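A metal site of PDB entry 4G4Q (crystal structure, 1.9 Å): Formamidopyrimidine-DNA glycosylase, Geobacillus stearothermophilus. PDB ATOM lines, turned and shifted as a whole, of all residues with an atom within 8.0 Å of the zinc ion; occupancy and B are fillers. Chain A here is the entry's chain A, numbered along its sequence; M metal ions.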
ATOM      1  N   PHE A 181      10.547   0.185 -25.946  1.00  0.00           N
ATOM      2  CA  PHE A 181      10.832  -1.033 -25.187  1.00  0.00           C
ATOM      3  C   PHE A 181      10.945  -2.238 -26.112  1.00  0.00           C
ATOM      4  O   PHE A 181      11.879  -3.036 -25.999  1.00  0.00           O
ATOM      5  CB  PHE A 181       9.786  -1.320 -24.111  1.00  0.00           C
ATOM      6  CG  PHE A 181       9.973  -2.673 -23.449  1.00  0.00           C
ATOM      7  CD1 PHE A 181      10.872  -2.823 -22.399  1.00  0.00           C
ATOM      8  CD2 PHE A 181       9.302  -3.791 -23.924  1.00  0.00           C
ATOM      9  CE1 PHE A 181      11.062  -4.065 -21.794  1.00  0.00           C
ATOM     10  CE2 PHE A 181       9.497  -5.035 -23.343  1.00  0.00           C
ATOM     11  CZ  PHE A 181      10.382  -5.176 -22.275  1.00  0.00           C
ATOM     12  N   TYR A 239       4.114  -3.294 -21.583  1.00  0.00           N
ATOM     13  CA  TYR A 239       5.409  -3.724 -21.052  1.00  0.00           C
ATOM     14  C   TYR A 239       5.995  -2.714 -20.070  1.00  0.00           C
ATOM     15  O   TYR A 239       6.605  -3.096 -19.070  1.00  0.00           O
ATOM     16  CB  TYR A 239       6.389  -3.924 -22.201  1.00  0.00           C
ATOM     17  CG  TYR A 239       6.061  -5.116 -23.056  1.00  0.00           C
ATOM     18  CD1 TYR A 239       5.574  -4.962 -24.353  1.00  0.00           C
ATOM     19  CD2 TYR A 239       6.246  -6.412 -22.560  1.00  0.00           C
ATOM     20  CE1 TYR A 239       5.274  -6.061 -25.131  1.00  0.00           C
ATOM     21  CE2 TYR A 239       5.946  -7.511 -23.338  1.00  0.00           C
ATOM     22  CZ  TYR A 239       5.459  -7.335 -24.624  1.00  0.00           C
ATOM     23  OH  TYR A 239       5.161  -8.420 -25.403  1.00  0.00           O
ATOM     24  N   VAL A 240       5.858  -1.428 -20.367  1.00  0.00           N
ATOM     25  CA  VAL A 240       6.526  -0.407 -19.546  1.00  0.00           C
ATOM     26  C   VAL A 240       5.622   0.748 -19.136  1.00  0.00           C
ATOM     27  O   VAL A 240       5.749   1.270 -18.024  1.00  0.00           O
ATOM     28  CB  VAL A 240       7.781   0.166 -20.231  1.00  0.00           C
ATOM     29  CG1 VAL A 240       8.859  -0.903 -20.359  1.00  0.00           C
ATOM     30  CG2 VAL A 240       7.446   0.769 -21.608  1.00  0.00           C
ATOM     31  N   PRO A 247       8.053  -5.218 -11.887  1.00  0.00           N
ATOM     32  CA  PRO A 247       9.049  -5.992 -12.627  1.00  0.00           C
ATOM     33  C   PRO A 247       8.803  -5.941 -14.132  1.00  0.00           C
ATOM     34  O   PRO A 247       7.666  -6.048 -14.590  1.00  0.00           O
ATOM     35  CB  PRO A 247       8.850  -7.412 -12.101  1.00  0.00           C
ATOM     36  CG  PRO A 247       8.195  -7.242 -10.766  1.00  0.00           C
ATOM     37  CD  PRO A 247       7.307  -6.053 -10.931  1.00  0.00           C
ATOM     38  N   CYS A 248       9.876  -5.785 -14.888  1.00  0.00           N
ATOM     39  CA  CYS A 248       9.773  -5.905 -16.342  1.00  0.00           C
ATOM     40  C   CYS A 248       9.206  -7.265 -16.681  1.00  0.00           C
ATOM     41  O   CYS A 248       9.596  -8.275 -16.092  1.00  0.00           O
ATOM     42  CB  CYS A 248      11.149  -5.736 -16.968  1.00  0.00           C
ATOM     43  SG  CYS A 248      11.210  -6.105 -18.727  1.00  0.00           S
ATOM     44  N   LYS A 249       8.289  -7.308 -17.647  1.00  0.00           N
ATOM     45  CA  LYS A 249       7.665  -8.584 -18.013  1.00  0.00           C
ATOM     46  C   LYS A 249       8.598  -9.541 -18.713  1.00  0.00           C
ATOM     47  O   LYS A 249       8.290 -10.735 -18.799  1.00  0.00           O
ATOM     48  CB  LYS A 249       6.415  -8.339 -18.869  1.00  0.00           C
ATOM     49  CG  LYS A 249       5.287  -7.765 -18.033  1.00  0.00           C
ATOM     50  CD  LYS A 249       4.027  -7.596 -18.839  1.00  0.00           C
ATOM     51  CE  LYS A 249       2.959  -6.915 -18.009  1.00  0.00           C
ATOM     52  NZ  LYS A 249       1.740  -6.629 -18.813  1.00  0.00           N
ATOM     53  N   ARG A 250       9.722  -9.022 -19.212  1.00  0.00           N
ATOM     54  CA  ARG A 250      10.693  -9.842 -19.908  1.00  0.00           C
ATOM     55  C   ARG A 250      11.945 -10.174 -19.087  1.00  0.00           C
ATOM     56  O   ARG A 250      12.560 -11.213 -19.311  1.00  0.00           O
ATOM     57  CB  ARG A 250      11.080  -9.218 -21.259  1.00  0.00           C
ATOM     58  CG  ARG A 250       9.934  -9.184 -22.245  1.00  0.00           C
ATOM     59  CD  ARG A 250      10.395  -9.136 -23.683  1.00  0.00           C
ATOM     60  NE  ARG A 250       9.265  -9.016 -24.599  1.00  0.00           N
ATOM     61  CZ  ARG A 250       9.339  -8.425 -25.786  1.00  0.00           C
ATOM     62  NH1 ARG A 250      10.480  -7.897 -26.204  1.00  0.00           N
ATOM     63  NH2 ARG A 250       8.255  -8.360 -26.558  1.00  0.00           N
ATOM     64  N   CYS A 251      12.330  -9.319 -18.131  1.00  0.00           N
ATOM     65  CA  CYS A 251      13.570  -9.596 -17.382  1.00  0.00           C
ATOM     66  C   CYS A 251      13.460  -9.454 -15.868  1.00  0.00           C
ATOM     67  O   CYS A 251      14.382  -9.808 -15.132  1.00  0.00           O
ATOM     68  CB  CYS A 251      14.725  -8.732 -17.903  1.00  0.00           C
ATOM     69  SG  CYS A 251      14.646  -7.014 -17.334  1.00  0.00           S
ATOM     70  N   GLY A 252      12.335  -8.927 -15.401  1.00  0.00           N
ATOM     71  CA  GLY A 252      12.092  -8.823 -13.968  1.00  0.00           C
ATOM     72  C   GLY A 252      12.712  -7.603 -13.300  1.00  0.00           C
ATOM     73  O   GLY A 252      12.492  -7.357 -12.121  1.00  0.00           O
ATOM     74  N   THR A 253      13.493  -6.841 -14.052  1.00  0.00           N
ATOM     75  CA  THR A 253      14.107  -5.628 -13.526  1.00  0.00           C
ATOM     76  C   THR A 253      13.033  -4.589 -13.267  1.00  0.00           C
ATOM     77  O   THR A 253      12.148  -4.415 -14.102  1.00  0.00           O
ATOM     78  CB  THR A 253      15.118  -5.054 -14.514  1.00  0.00           C
ATOM     79  OG1 THR A 253      16.212  -5.975 -14.637  1.00  0.00           O
ATOM     80  CG2 THR A 253      15.643  -3.697 -14.033  1.00  0.00           C
ATOM     81  N   PRO A 254      13.082  -3.878 -12.126  1.00  0.00           N
ATOM     82  CA  PRO A 254      12.035  -2.879 -11.915  1.00  0.00           C
ATOM     83  C   PRO A 254      11.995  -1.844 -13.041  1.00  0.00           C
ATOM     84  O   PRO A 254      13.025  -1.316 -13.428  1.00  0.00           O
ATOM     85  CB  PRO A 254      12.446  -2.196 -10.594  1.00  0.00           C
ATOM     86  CG  PRO A 254      13.268  -3.258  -9.872  1.00  0.00           C
ATOM     87  CD  PRO A 254      14.012  -3.977 -10.979  1.00  0.00           C
ATOM     88  N   ILE A 255      10.798  -1.590 -13.566  1.00  0.00           N
ATOM     89  CA  ILE A 255      10.628  -0.578 -14.596  1.00  0.00           C
ATOM     90  C   ILE A 255      10.876   0.777 -13.968  1.00  0.00           C
ATOM     91  O   ILE A 255      10.516   1.010 -12.810  1.00  0.00           O
ATOM     92  CB  ILE A 255       9.236  -0.656 -15.242  1.00  0.00           C
ATOM     93  CG1 ILE A 255       9.088  -1.978 -15.985  1.00  0.00           C
ATOM     94  CG2 ILE A 255       8.984   0.557 -16.174  1.00  0.00           C
ATOM     95  CD1 ILE A 255      10.193  -2.239 -17.040  1.00  0.00           C
ATOM     96  N   TYR A 267      10.727   2.855 -18.925  1.00  0.00           N
ATOM     97  CA  TYR A 267      11.633   2.000 -19.645  1.00  0.00           C
ATOM     98  C   TYR A 267      12.211   0.941 -18.726  1.00  0.00           C
ATOM     99  O   TYR A 267      12.212   1.084 -17.501  1.00  0.00           O
ATOM    100  CB  TYR A 267      12.768   2.819 -20.257  1.00  0.00           C
ATOM    101  CG  TYR A 267      13.588   3.568 -19.225  1.00  0.00           C
ATOM    102  CD1 TYR A 267      14.751   3.012 -18.698  1.00  0.00           C
ATOM    103  CD2 TYR A 267      13.176   4.809 -18.743  1.00  0.00           C
ATOM    104  CE1 TYR A 267      15.485   3.675 -17.735  1.00  0.00           C
ATOM    105  CE2 TYR A 267      13.911   5.487 -17.781  1.00  0.00           C
ATOM    106  CZ  TYR A 267      15.065   4.909 -17.283  1.00  0.00           C
ATOM    107  OH  TYR A 267      15.810   5.557 -16.326  1.00  0.00           O
ATOM    108  N   CYS A 268      12.677  -0.135 -19.322  1.00  0.00           N
ATOM    109  CA  CYS A 268      13.445  -1.096 -18.561  1.00  0.00           C
ATOM    110  C   CYS A 268      14.923  -0.814 -18.802  1.00  0.00           C
ATOM    111  O   CYS A 268      15.397  -0.818 -19.957  1.00  0.00           O
ATOM    112  CB  CYS A 268      13.086  -2.521 -18.992  1.00  0.00           C
ATOM    113  SG  CYS A 268      14.183  -3.656 -18.205  1.00  0.00           S
ATOM    114  N   PRO A 269      15.667  -0.524 -17.727  1.00  0.00           N
ATOM    115  CA  PRO A 269      17.076  -0.136 -17.865  1.00  0.00           C
ATOM    116  C   PRO A 269      17.943  -1.315 -18.280  1.00  0.00           C
ATOM    117  O   PRO A 269      19.117  -1.128 -18.596  1.00  0.00           O
ATOM    118  CB  PRO A 269      17.463   0.340 -16.469  1.00  0.00           C
ATOM    119  CG  PRO A 269      16.572  -0.430 -15.552  1.00  0.00           C
ATOM    120  CD  PRO A 269      15.251  -0.571 -16.310  1.00  0.00           C
ATOM    121  N   ARG A 270      17.378  -2.514 -18.240  1.00  0.00           N
ATOM    122  CA  ARG A 270      18.120  -3.693 -18.682  1.00  0.00           C
ATOM    123  C   ARG A 270      17.805  -4.074 -20.136  1.00  0.00           C
ATOM    124  O   ARG A 270      18.717  -4.306 -20.929  1.00  0.00           O
ATOM    125  CB  ARG A 270      17.862  -4.880 -17.746  1.00  0.00           C
ATOM    126  CG  ARG A 270      18.621  -6.130 -18.131  1.00  0.00           C
ATOM    127  CD  ARG A 270      18.420  -7.248 -17.099  1.00  0.00           C
ATOM    128  NE  ARG A 270      19.250  -8.377 -17.473  1.00  0.00           N
ATOM    129  CZ  ARG A 270      19.406  -9.473 -16.738  1.00  0.00           C
ATOM    130  NH1 ARG A 270      20.196 -10.430 -17.179  1.00  0.00           N
ATOM    131  NH2 ARG A 270      18.791  -9.600 -15.559  1.00  0.00           N
ATOM    132  N   CYS A 271      16.515  -4.121 -20.486  1.00  0.00           N
ATOM    133  CA  CYS A 271      16.102  -4.472 -21.857  1.00  0.00           C
ATOM    134  C   CYS A 271      16.415  -3.396 -22.877  1.00  0.00           C
ATOM    135  O   CYS A 271      16.653  -3.694 -24.054  1.00  0.00           O
ATOM    136  CB  CYS A 271      14.581  -4.792 -21.919  1.00  0.00           C
ATOM    137  SG  CYS A 271      14.130  -6.359 -21.070  1.00  0.00           S
ATOM    138  N   GLN A 272      16.420  -2.150 -22.454  1.00  0.00           N
ATOM    139  CA  GLN A 272      16.623  -1.057 -23.409  1.00  0.00           C
ATOM    140  C   GLN A 272      18.041  -0.515 -23.283  1.00  0.00           C
ATOM    141  O   GLN A 272      18.542  -0.352 -22.180  1.00  0.00           O
ATOM    142  CB  GLN A 272      15.583   0.019 -23.189  1.00  0.00           C
ATOM    143  CG  GLN A 272      14.199  -0.448 -23.609  1.00  0.00           C
ATOM    144  CD  GLN A 272      13.131   0.465 -23.121  1.00  0.00           C
ATOM    145  OE1 GLN A 272      12.474   0.171 -22.125  1.00  0.00           O
ATOM    146  NE2 GLN A 272      12.940   1.604 -23.794  1.00  0.00           N
HETATM  147 ZN    ZN M   1      13.527  -5.760 -18.977  1.00  0.00          ZN
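The side-chain sulfur (SG) of Cys 268 sits close to the backbone NH (N) of Arg 270, at 3.4 Å. The backbone NH (N) of Cys 268 sits at hydrogen-bond distance from the side-chain amide oxygen (OE1) of Gln 272. The side-chain sulfur (SG) of Cys 251 lies close to the side-chain hydroxyl (OG1) of Thr 253 (3.3 Å). The side-chain sulfur of Cys 248 lies close to the backbone NH of Arg 250 (3.3 Å). O of Thr 253 lies within hydrogen-bond range of N of Cys 248 (2.8 Å).
Four residues have an atom within 4 Å of the zinc ion: Cys 248, Cys 251, Cys 268 and Cys 271. The nearest printed residue that does not touch the zinc ion is Phe 181 (4.1 Å).
SG of Cys 271 is bound to the zinc ion (2.3 Å). SG of Cys 268 is bound to the zinc ion (2.3 Å). SG of Cys 251 binds the zinc ion (2.4 Å). The zinc ion is bound by the side-chain sulfur (SG) of Cys 248 (2.4 Å).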
